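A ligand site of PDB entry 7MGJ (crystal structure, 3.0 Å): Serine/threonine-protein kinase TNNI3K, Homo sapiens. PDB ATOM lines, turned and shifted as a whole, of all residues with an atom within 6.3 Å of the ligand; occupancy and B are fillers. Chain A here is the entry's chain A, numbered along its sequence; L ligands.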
ATOM      1  N   ILE A  69      23.744   1.216 -16.552  1.00  0.00           N
ATOM      2  CA  ILE A  69      24.582   2.402 -16.327  1.00  0.00           C
ATOM      3  C   ILE A  69      24.863   2.626 -14.830  1.00  0.00           C
ATOM      4  O   ILE A  69      25.897   3.211 -14.452  1.00  0.00           O
ATOM      5  CB  ILE A  69      23.878   3.692 -16.810  1.00  0.00           C
ATOM      6  CG1 ILE A  69      23.423   3.601 -18.256  1.00  0.00           C
ATOM      7  CG2 ILE A  69      24.790   4.895 -16.702  1.00  0.00           C
ATOM      8  CD1 ILE A  69      22.647   4.838 -18.673  1.00  0.00           C
ATOM      9  N   VAL A  77      19.805   1.491 -13.544  1.00  0.00           N
ATOM     10  CA  VAL A  77      19.689   2.526 -14.564  1.00  0.00           C
ATOM     11  C   VAL A  77      20.248   1.986 -15.879  1.00  0.00           C
ATOM     12  O   VAL A  77      21.421   1.616 -15.987  1.00  0.00           O
ATOM     13  CB  VAL A  77      20.464   3.818 -14.164  1.00  0.00           C
ATOM     14  CG1 VAL A  77      20.201   4.942 -15.181  1.00  0.00           C
ATOM     15  CG2 VAL A  77      20.072   4.271 -12.772  1.00  0.00           C
ATOM     16  N   TYR A  78      19.402   1.908 -16.904  1.00  0.00           N
ATOM     17  CA  TYR A  78      19.849   1.372 -18.182  1.00  0.00           C
ATOM     18  C   TYR A  78      20.075   2.452 -19.242  1.00  0.00           C
ATOM     19  O   TYR A  78      19.435   3.510 -19.237  1.00  0.00           O
ATOM     20  CB  TYR A  78      18.835   0.362 -18.716  1.00  0.00           C
ATOM     21  CG  TYR A  78      18.588  -0.862 -17.844  1.00  0.00           C
ATOM     22  CD1 TYR A  78      17.719  -0.798 -16.758  1.00  0.00           C
ATOM     23  CD2 TYR A  78      19.187  -2.081 -18.122  1.00  0.00           C
ATOM     24  CE1 TYR A  78      17.473  -1.922 -15.969  1.00  0.00           C
ATOM     25  CE2 TYR A  78      18.953  -3.196 -17.347  1.00  0.00           C
ATOM     26  CZ  TYR A  78      18.096  -3.111 -16.267  1.00  0.00           C
ATOM     27  OH  TYR A  78      17.849  -4.223 -15.485  1.00  0.00           O
ATOM     28  N   ALA A  88      17.747   6.985 -21.460  1.00  0.00           N
ATOM     29  CA  ALA A  88      18.219   6.422 -20.188  1.00  0.00           C
ATOM     30  C   ALA A  88      16.995   5.938 -19.433  1.00  0.00           C
ATOM     31  O   ALA A  88      16.033   6.681 -19.252  1.00  0.00           O
ATOM     32  CB  ALA A  88      18.981   7.473 -19.375  1.00  0.00           C
ATOM     33  N   ILE A  89      17.008   4.677 -19.024  1.00  0.00           N
ATOM     34  CA  ILE A  89      15.801   4.179 -18.382  1.00  0.00           C
ATOM     35  C   ILE A  89      16.077   3.897 -16.937  1.00  0.00           C
ATOM     36  O   ILE A  89      16.975   3.127 -16.612  1.00  0.00           O
ATOM     37  CB  ILE A  89      15.258   2.920 -19.047  1.00  0.00           C
ATOM     38  CG1 ILE A  89      15.125   3.146 -20.550  1.00  0.00           C
ATOM     39  CG2 ILE A  89      13.920   2.524 -18.395  1.00  0.00           C
ATOM     40  CD1 ILE A  89      16.251   2.529 -21.337  1.00  0.00           C
ATOM     41  N   LYS A  90      15.299   4.553 -16.083  1.00  0.00           N
ATOM     42  CA  LYS A  90      15.398   4.388 -14.645  1.00  0.00           C
ATOM     43  C   LYS A  90      14.313   3.376 -14.289  1.00  0.00           C
ATOM     44  O   LYS A  90      13.128   3.710 -14.261  1.00  0.00           O
ATOM     45  CB  LYS A  90      15.123   5.732 -13.967  1.00  0.00           C
ATOM     46  CG  LYS A  90      16.028   6.107 -12.799  1.00  0.00           C
ATOM     47  CD  LYS A  90      15.267   6.952 -11.792  1.00  0.00           C
ATOM     48  CE  LYS A  90      16.194   7.692 -10.842  1.00  0.00           C
ATOM     49  NZ  LYS A  90      16.489   9.070 -11.348  1.00  0.00           N
ATOM     50  N   GLU A 109       8.886  11.539  -8.555  1.00  0.00           N
ATOM     51  CA  GLU A 109       9.803  11.811  -9.661  1.00  0.00           C
ATOM     52  C   GLU A 109       9.058  12.117 -10.972  1.00  0.00           C
ATOM     53  O   GLU A 109       9.372  13.107 -11.639  1.00  0.00           O
ATOM     54  CB  GLU A 109      10.801  10.681  -9.856  1.00  0.00           C
ATOM     55  CG  GLU A 109      11.953  11.084 -10.757  1.00  0.00           C
ATOM     56  CD  GLU A 109      13.071  10.061 -10.759  1.00  0.00           C
ATOM     57  OE1 GLU A 109      12.877   8.998 -10.123  1.00  0.00           O
ATOM     58  OE2 GLU A 109      14.128  10.321 -11.392  1.00  0.00           O
ATOM     59  N   ILE A 112       7.493  15.459 -10.954  1.00  0.00           N
ATOM     60  CA  ILE A 112       8.515  16.476 -11.198  1.00  0.00           C
ATOM     61  C   ILE A 112       8.856  16.533 -12.703  1.00  0.00           C
ATOM     62  O   ILE A 112       8.927  17.616 -13.303  1.00  0.00           O
ATOM     63  CB  ILE A 112       9.840  16.184 -10.406  1.00  0.00           C
ATOM     64  CG1 ILE A 112       9.629  16.176  -8.886  1.00  0.00           C
ATOM     65  CG2 ILE A 112      10.884  17.255 -10.683  1.00  0.00           C
ATOM     66  CD1 ILE A 112       9.256  17.519  -8.326  1.00  0.00           C
ATOM     67  N   LEU A 113       9.076  15.361 -13.289  1.00  0.00           N
ATOM     68  CA  LEU A 113       9.582  15.270 -14.655  1.00  0.00           C
ATOM     69  C   LEU A 113       8.625  15.770 -15.759  1.00  0.00           C
ATOM     70  O   LEU A 113       9.091  16.292 -16.775  1.00  0.00           O
ATOM     71  CB  LEU A 113      10.061  13.848 -14.949  1.00  0.00           C
ATOM     72  CG  LEU A 113      11.393  13.473 -14.264  1.00  0.00           C
ATOM     73  CD1 LEU A 113      11.760  12.017 -14.473  1.00  0.00           C
ATOM     74  CD2 LEU A 113      12.522  14.378 -14.739  1.00  0.00           C
ATOM     75  N   LEU A 116       9.159  19.593 -16.405  1.00  0.00           N
ATOM     76  CA  LEU A 116      10.440  20.214 -16.751  1.00  0.00           C
ATOM     77  C   LEU A 116      10.590  20.453 -18.234  1.00  0.00           C
ATOM     78  O   LEU A 116      10.626  19.516 -19.022  1.00  0.00           O
ATOM     79  CB  LEU A 116      11.616  19.381 -16.266  1.00  0.00           C
ATOM     80  CG  LEU A 116      11.588  18.982 -14.795  1.00  0.00           C
ATOM     81  CD1 LEU A 116      12.845  18.195 -14.475  1.00  0.00           C
ATOM     82  CD2 LEU A 116      11.405  20.211 -13.917  1.00  0.00           C
ATOM     83  N   VAL A 121      18.033  21.480 -18.171  1.00  0.00           N
ATOM     84  CA  VAL A 121      17.481  20.503 -17.260  1.00  0.00           C
ATOM     85  C   VAL A 121      17.111  19.235 -18.030  1.00  0.00           C
ATOM     86  O   VAL A 121      16.642  19.313 -19.169  1.00  0.00           O
ATOM     87  CB  VAL A 121      16.251  21.065 -16.542  1.00  0.00           C
ATOM     88  CG1 VAL A 121      15.610  20.021 -15.650  1.00  0.00           C
ATOM     89  CG2 VAL A 121      16.626  22.288 -15.722  1.00  0.00           C
ATOM     90  N   ILE A 122      17.335  18.087 -17.390  1.00  0.00           N
ATOM     91  CA  ILE A 122      17.115  16.796 -18.026  1.00  0.00           C
ATOM     92  C   ILE A 122      15.751  16.696 -18.722  1.00  0.00           C
ATOM     93  O   ILE A 122      14.775  17.308 -18.282  1.00  0.00           O
ATOM     94  CB  ILE A 122      17.321  15.653 -17.011  1.00  0.00           C
ATOM     95  CG1 ILE A 122      17.512  14.332 -17.750  1.00  0.00           C
ATOM     96  CG2 ILE A 122      16.166  15.588 -16.026  1.00  0.00           C
ATOM     97  CD1 ILE A 122      18.024  13.217 -16.876  1.00  0.00           C
ATOM     98  N   ILE A 137      11.132   4.934 -15.874  1.00  0.00           N
ATOM     99  CA  ILE A 137      11.233   6.332 -16.211  1.00  0.00           C
ATOM    100  C   ILE A 137      12.264   6.477 -17.315  1.00  0.00           C
ATOM    101  O   ILE A 137      13.373   5.950 -17.209  1.00  0.00           O
ATOM    102  CB  ILE A 137      11.606   7.172 -14.975  1.00  0.00           C
ATOM    103  CG1 ILE A 137      10.361   7.388 -14.108  1.00  0.00           C
ATOM    104  CG2 ILE A 137      12.203   8.517 -15.367  1.00  0.00           C
ATOM    105  CD1 ILE A 137      10.651   7.867 -12.719  1.00  0.00           C
ATOM    106  N   VAL A 138      11.877   7.170 -18.382  1.00  0.00           N
ATOM    107  CA  VAL A 138      12.721   7.299 -19.558  1.00  0.00           C
ATOM    108  C   VAL A 138      13.104   8.748 -19.774  1.00  0.00           C
ATOM    109  O   VAL A 138      12.250   9.633 -19.776  1.00  0.00           O
ATOM    110  CB  VAL A 138      12.015   6.772 -20.811  1.00  0.00           C
ATOM    111  CG1 VAL A 138      12.944   6.813 -22.013  1.00  0.00           C
ATOM    112  CG2 VAL A 138      11.508   5.379 -20.564  1.00  0.00           C
ATOM    113  N   THR A 139      14.388   9.012 -19.950  1.00  0.00           N
ATOM    114  CA  THR A 139      14.803  10.385 -20.202  1.00  0.00           C
ATOM    115  C   THR A 139      15.811  10.400 -21.351  1.00  0.00           C
ATOM    116  O   THR A 139      16.226   9.339 -21.855  1.00  0.00           O
ATOM    117  CB  THR A 139      15.497  10.978 -18.990  1.00  0.00           C
ATOM    118  OG1 THR A 139      16.810  10.429 -18.883  1.00  0.00           O
ATOM    119  CG2 THR A 139      14.699  10.710 -17.716  1.00  0.00           C
ATOM    120  N   GLN A 140      16.241  11.580 -21.762  1.00  0.00           N
ATOM    121  CA  GLN A 140      17.324  11.680 -22.729  1.00  0.00           C
ATOM    122  C   GLN A 140      18.584  11.035 -22.180  1.00  0.00           C
ATOM    123  O   GLN A 140      18.697  10.765 -20.976  1.00  0.00           O
ATOM    124  CB  GLN A 140      17.604  13.125 -23.099  1.00  0.00           C
ATOM    125  CG  GLN A 140      17.831  14.054 -21.889  1.00  0.00           C
ATOM    126  CD  GLN A 140      18.335  15.429 -22.285  1.00  0.00           C
ATOM    127  OE1 GLN A 140      17.952  16.440 -21.682  1.00  0.00           O
ATOM    128  NE2 GLN A 140      19.192  15.469 -23.314  1.00  0.00           N
ATOM    129  N   TYR A 141      19.514  10.708 -23.056  1.00  0.00           N
ATOM    130  CA  TYR A 141      20.788  10.184 -22.638  1.00  0.00           C
ATOM    131  C   TYR A 141      21.798  11.252 -23.038  1.00  0.00           C
ATOM    132  O   TYR A 141      21.979  11.532 -24.228  1.00  0.00           O
ATOM    133  CB  TYR A 141      21.063   8.840 -23.316  1.00  0.00           C
ATOM    134  CG  TYR A 141      22.416   8.211 -23.031  1.00  0.00           C
ATOM    135  CD1 TYR A 141      22.587   7.356 -21.949  1.00  0.00           C
ATOM    136  CD2 TYR A 141      23.517   8.452 -23.846  1.00  0.00           C
ATOM    137  CE1 TYR A 141      23.806   6.764 -21.669  1.00  0.00           C
ATOM    138  CE2 TYR A 141      24.749   7.869 -23.594  1.00  0.00           C
ATOM    139  CZ  TYR A 141      24.896   7.021 -22.498  1.00  0.00           C
ATOM    140  OH  TYR A 141      26.127   6.413 -22.219  1.00  0.00           O
ATOM    141  N   ILE A 142      22.438  11.876 -22.047  1.00  0.00           N
ATOM    142  CA  ILE A 142      23.451  12.884 -22.335  1.00  0.00           C
ATOM    143  C   ILE A 142      24.791  12.166 -22.343  1.00  0.00           C
ATOM    144  O   ILE A 142      25.248  11.701 -21.303  1.00  0.00           O
ATOM    145  CB  ILE A 142      23.459  14.035 -21.293  1.00  0.00           C
ATOM    146  CG1 ILE A 142      22.134  14.815 -21.291  1.00  0.00           C
ATOM    147  CG2 ILE A 142      24.504  15.004 -21.623  1.00  0.00           C
ATOM    148  CD1 ILE A 142      21.141  14.397 -20.198  1.00  0.00           C
ATOM    149  N   SER A 143      25.389  12.046 -23.542  1.00  0.00           N
ATOM    150  CA  SER A 143      26.484  11.076 -23.813  1.00  0.00           C
ATOM    151  C   SER A 143      27.866  11.449 -23.310  1.00  0.00           C
ATOM    152  O   SER A 143      28.756  10.593 -23.242  1.00  0.00           O
ATOM    153  CB  SER A 143      26.581  10.762 -25.302  1.00  0.00           C
ATOM    154  OG  SER A 143      27.108  11.849 -26.014  1.00  0.00           O
ATOM    155  N   GLY A 144      28.041  12.715 -22.938  1.00  0.00           N
ATOM    156  CA  GLY A 144      29.328  13.192 -22.465  1.00  0.00           C
ATOM    157  C   GLY A 144      29.681  12.867 -21.025  1.00  0.00           C
ATOM    158  O   GLY A 144      30.772  13.208 -20.592  1.00  0.00           O
ATOM    159  N   GLY A 145      28.775  12.209 -20.279  1.00  0.00           N
ATOM    160  CA  GLY A 145      29.029  11.784 -18.902  1.00  0.00           C
ATOM    161  C   GLY A 145      28.848  12.843 -17.836  1.00  0.00           C
ATOM    162  O   GLY A 145      28.378  13.949 -18.141  1.00  0.00           O
ATOM    163  N   SER A 146      29.221  12.543 -16.599  1.00  0.00           N
ATOM    164  CA  SER A 146      29.041  13.502 -15.492  1.00  0.00           C
ATOM    165  C   SER A 146      30.176  14.509 -15.434  1.00  0.00           C
ATOM    166  O   SER A 146      31.293  14.241 -15.897  1.00  0.00           O
ATOM    167  CB  SER A 146      28.969  12.807 -14.135  1.00  0.00           C
ATOM    168  OG  SER A 146      30.215  12.210 -13.805  1.00  0.00           O
ATOM    169  N   LEU A 177      14.557  25.847 -12.155  1.00  0.00           N
ATOM    170  CA  LEU A 177      13.916  25.004 -11.146  1.00  0.00           C
ATOM    171  C   LEU A 177      13.346  25.870 -10.045  1.00  0.00           C
ATOM    172  O   LEU A 177      12.284  25.567  -9.520  1.00  0.00           O
ATOM    173  CB  LEU A 177      14.863  23.962 -10.569  1.00  0.00           C
ATOM    174  CG  LEU A 177      15.385  22.825 -11.459  1.00  0.00           C
ATOM    175  CD1 LEU A 177      16.490  22.054 -10.742  1.00  0.00           C
ATOM    176  CD2 LEU A 177      14.260  21.909 -11.790  1.00  0.00           C
ATOM    177  N   ILE A 184      11.250  24.191  -6.946  1.00  0.00           N
ATOM    178  CA  ILE A 184      11.816  22.907  -6.597  1.00  0.00           C
ATOM    179  C   ILE A 184      13.185  23.098  -5.970  1.00  0.00           C
ATOM    180  O   ILE A 184      14.070  23.692  -6.597  1.00  0.00           O
ATOM    181  CB  ILE A 184      12.022  22.016  -7.829  1.00  0.00           C
ATOM    182  CG1 ILE A 184      10.691  21.567  -8.367  1.00  0.00           C
ATOM    183  CG2 ILE A 184      12.811  20.788  -7.468  1.00  0.00           C
ATOM    184  CD1 ILE A 184      10.826  20.710  -9.580  1.00  0.00           C
ATOM    185  N   HIS A 186      16.462  21.396  -5.332  1.00  0.00           N
ATOM    186  CA  HIS A 186      17.164  20.238  -5.866  1.00  0.00           C
ATOM    187  C   HIS A 186      17.670  19.348  -4.748  1.00  0.00           C
ATOM    188  O   HIS A 186      17.561  18.124  -4.840  1.00  0.00           O
ATOM    189  CB  HIS A 186      18.338  20.682  -6.752  1.00  0.00           C
ATOM    190  CG  HIS A 186      19.013  19.551  -7.471  1.00  0.00           C
ATOM    191  ND1 HIS A 186      19.648  18.526  -6.802  1.00  0.00           N
ATOM    192  CD2 HIS A 186      19.153  19.284  -8.786  1.00  0.00           C
ATOM    193  CE1 HIS A 186      20.155  17.678  -7.679  1.00  0.00           C
ATOM    194  NE2 HIS A 186      19.870  18.107  -8.888  1.00  0.00           N
ATOM    195  N   LEU A 195      25.279  16.660 -15.835  1.00  0.00           N
ATOM    196  CA  LEU A 195      25.704  15.934 -17.032  1.00  0.00           C
ATOM    197  C   LEU A 195      26.181  16.851 -18.154  1.00  0.00           C
ATOM    198  O   LEU A 195      25.762  18.024 -18.250  1.00  0.00           O
ATOM    199  CB  LEU A 195      24.568  15.057 -17.512  1.00  0.00           C
ATOM    200  CG  LEU A 195      24.127  14.117 -16.390  1.00  0.00           C
ATOM    201  CD1 LEU A 195      22.715  13.613 -16.663  1.00  0.00           C
ATOM    202  CD2 LEU A 195      25.144  12.982 -16.257  1.00  0.00           C
ATOM    203  N   VAL A 204      21.309  19.767 -15.813  1.00  0.00           N
ATOM    204  CA  VAL A 204      21.171  19.449 -14.402  1.00  0.00           C
ATOM    205  C   VAL A 204      20.188  18.348 -14.193  1.00  0.00           C
ATOM    206  O   VAL A 204      19.067  18.474 -14.526  1.00  0.00           O
ATOM    207  CB  VAL A 204      20.715  20.658 -13.587  1.00  0.00           C
ATOM    208  CG1 VAL A 204      20.524  20.288 -12.137  1.00  0.00           C
ATOM    209  CG2 VAL A 204      21.738  21.753 -13.674  1.00  0.00           C
ATOM    210  N   ALA A 205      20.624  17.297 -13.555  1.00  0.00           N
ATOM    211  CA  ALA A 205      19.776  16.148 -13.362  1.00  0.00           C
ATOM    212  C   ALA A 205      19.868  15.652 -11.936  1.00  0.00           C
ATOM    213  O   ALA A 205      20.593  16.212 -11.120  1.00  0.00           O
ATOM    214  CB  ALA A 205      20.154  15.065 -14.299  1.00  0.00           C
ATOM    215  N   ASP A 206      19.140  14.595 -11.636  1.00  0.00           N
ATOM    216  CA  ASP A 206      19.188  13.989 -10.307  1.00  0.00           C
ATOM    217  C   ASP A 206      19.135  12.482 -10.430  1.00  0.00           C
ATOM    218  O   ASP A 206      18.112  11.917 -10.800  1.00  0.00           O
ATOM    219  CB  ASP A 206      18.006  14.465  -9.469  1.00  0.00           C
ATOM    220  CG  ASP A 206      18.112  14.042  -8.013  1.00  0.00           C
ATOM    221  OD1 ASP A 206      18.911  13.134  -7.689  1.00  0.00           O
ATOM    222  OD2 ASP A 206      17.390  14.638  -7.179  1.00  0.00           O
ATOM    223  N   PHE A 207      20.232  11.824 -10.094  1.00  0.00           N
ATOM    224  CA  PHE A 207      20.286  10.361 -10.183  1.00  0.00           C
ATOM    225  C   PHE A 207      19.483   9.647  -9.115  1.00  0.00           C
ATOM    226  O   PHE A 207      19.460   8.416  -9.076  1.00  0.00           O
ATOM    227  CB  PHE A 207      21.724   9.854 -10.189  1.00  0.00           C
ATOM    228  CG  PHE A 207      22.305   9.806 -11.550  1.00  0.00           C
ATOM    229  CD1 PHE A 207      23.117  10.836 -12.017  1.00  0.00           C
ATOM    230  CD2 PHE A 207      21.991   8.741 -12.421  1.00  0.00           C
ATOM    231  CE1 PHE A 207      23.642  10.785 -13.310  1.00  0.00           C
ATOM    232  CE2 PHE A 207      22.516   8.677 -13.707  1.00  0.00           C
ATOM    233  CZ  PHE A 207      23.351   9.700 -14.159  1.00  0.00           C
ATOM    234  N   GLY A 208      18.863  10.409  -8.231  1.00  0.00           N
ATOM    235  CA  GLY A 208      17.937   9.853  -7.258  1.00  0.00           C
ATOM    236  C   GLY A 208      18.694   9.138  -6.174  1.00  0.00           C
ATOM    237  O   GLY A 208      18.106   8.332  -5.466  1.00  0.00           O
HETATM  238  N1  LIG L   1      25.078   9.381 -19.783  1.00  0.00           N
HETATM  239  C1  LIG L   1      24.501   8.764 -18.689  1.00  0.00           C
HETATM  240  O1  LIG L   1      20.496   8.695 -15.996  1.00  0.00           O
HETATM  241  C2  LIG L   1      23.152   9.280 -18.360  1.00  0.00           C
HETATM  242  O2  LIG L   1      17.178  13.404 -13.159  1.00  0.00           O
HETATM  243  C3  LIG L   1      22.465   8.730 -17.305  1.00  0.00           C
HETATM  244  C4  LIG L   1      21.206   9.238 -17.050  1.00  0.00           C
HETATM  245  C5  LIG L   1      19.660  10.529 -14.662  1.00  0.00           C
HETATM  246  C6  LIG L   1      18.585  11.168 -14.085  1.00  0.00           C
HETATM  247  C7  LIG L   1      17.288  10.689 -14.239  1.00  0.00           C
HETATM  248  C8  LIG L   1      16.244  12.614 -13.091  1.00  0.00           C
HETATM  249  C9  LIG L   1      14.931  14.064 -11.673  1.00  0.00           C
HETATM  250  C10 LIG L   1      14.190  13.989 -10.520  1.00  0.00           C
HETATM  251  C11 LIG L   1      14.010  15.118  -9.749  1.00  0.00           C
HETATM  252  C12 LIG L   1      14.575  16.314 -10.118  1.00  0.00           C
HETATM  253  C13 LIG L   1      15.316  16.378 -11.279  1.00  0.00           C
HETATM  254  C14 LIG L   1      15.497  15.261 -12.056  1.00  0.00           C
HETATM  255  C15 LIG L   1      15.933  17.662 -11.693  1.00  0.00           C
HETATM  256  C16 LIG L   1      17.074   9.564 -14.985  1.00  0.00           C
HETATM  257  C17 LIG L   1      20.692  10.241 -17.834  1.00  0.00           C
HETATM  258  C18 LIG L   1      21.467  10.708 -18.865  1.00  0.00           C
HETATM  259  C19 LIG L   1      26.450   9.095 -20.121  1.00  0.00           C
HETATM  260  O3  LIG L   1      25.019   7.862 -18.045  1.00  0.00           O
HETATM  261  C20 LIG L   1      19.441   9.400 -15.416  1.00  0.00           C
HETATM  262  N2  LIG L   1      16.182  11.331 -13.642  1.00  0.00           N
HETATM  263  N3  LIG L   1      15.083  12.902 -12.431  1.00  0.00           N
HETATM  264  F1  LIG L   1      15.083  18.715 -11.508  1.00  0.00           F
HETATM  265  F2  LIG L   1      17.090  17.931 -11.011  1.00  0.00           F
HETATM  266  F3  LIG L   1      16.307  17.660 -13.000  1.00  0.00           F
HETATM  267  C21 LIG L   1      18.155   8.930 -15.556  1.00  0.00           C
HETATM  268  N4  LIG L   1      22.691  10.260 -19.156  1.00  0.00           N
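A nitrogen (N2) of the ligand sits close to the side-chain amino group (NZ) of Lys 90 (3.2 Å). O of Val 204 lies close to F3 of the ligand (3.3 Å). Merely in contact with the ligand: Phe 207, Ile 69, Leu 177, His 186, Tyr 141, Gln 140, Ile 122, Ala 205, Ala 88, Val 121, Leu 113, Leu 116, Thr 139, Ile 112, Val 77, Leu 195 and Gly 145. Hydrophobic or aromatic side chains within 4 Å of the ligand: Ile 69, Val 77, Ala 88, Ile 112, Leu 113, Leu 116, Val 121, Ile 122, Tyr 141, Ile 142, Leu 177, His 186, Leu 195, Ala 205 and Phe 207. Of the 31 residues printed, 22 come within 4 Å of the ligand. The nearest printed residue that does not touch the ligand is Ser 143 (4.2 Å).
The backbone NH (N) of Asp 206 lies within hydrogen-bond range of an oxygen (O2) of the ligand, 2.8 Å away. N2 of the ligand sits close to O of Asp 206, 3.5 Å away. N of Ile 142 lies within hydrogen-bond range of N4 of the ligand, at 3.3 Å. A nitrogen (N1) of the ligand is in hydrogen-bond range of the backbone carbonyl oxygen (O) of Ile 142. N3 of the ligand lies within hydrogen-bond range of OE2 of Glu 109 (2.9 Å).
O of Asp 206 sits at hydrogen-bond distance from NZ of Lys 90 (3.3 Å). N of Gly 208 is in hydrogen-bond range of OD1 of Asp 206, at 2.8 Å. OE2 of Glu 109 is in salt-bridge range of NZ of Lys 90. The backbone NH of Lys 90 lies within hydrogen-bond range of the backbone carbonyl oxygen of Ile 137 (2.6 Å). The backbone carbonyl oxygen (O) of Val 204 is in hydrogen-bond range of the backbone NH (N) of Ile 122. The backbone carbonyl oxygen (O) of Val 77 lies within hydrogen-bond range of the backbone NH (N) of Ile 69 (2.4 Å). A ring nitrogen (NE2) of His 186 lies within hydrogen-bond range of the backbone carbonyl oxygen (O) of Ala 205 (3.0 Å). The backbone NH (N) of Ala 88 sits at hydrogen-bond distance from the backbone carbonyl oxygen (O) of Thr 139 (2.8 Å).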
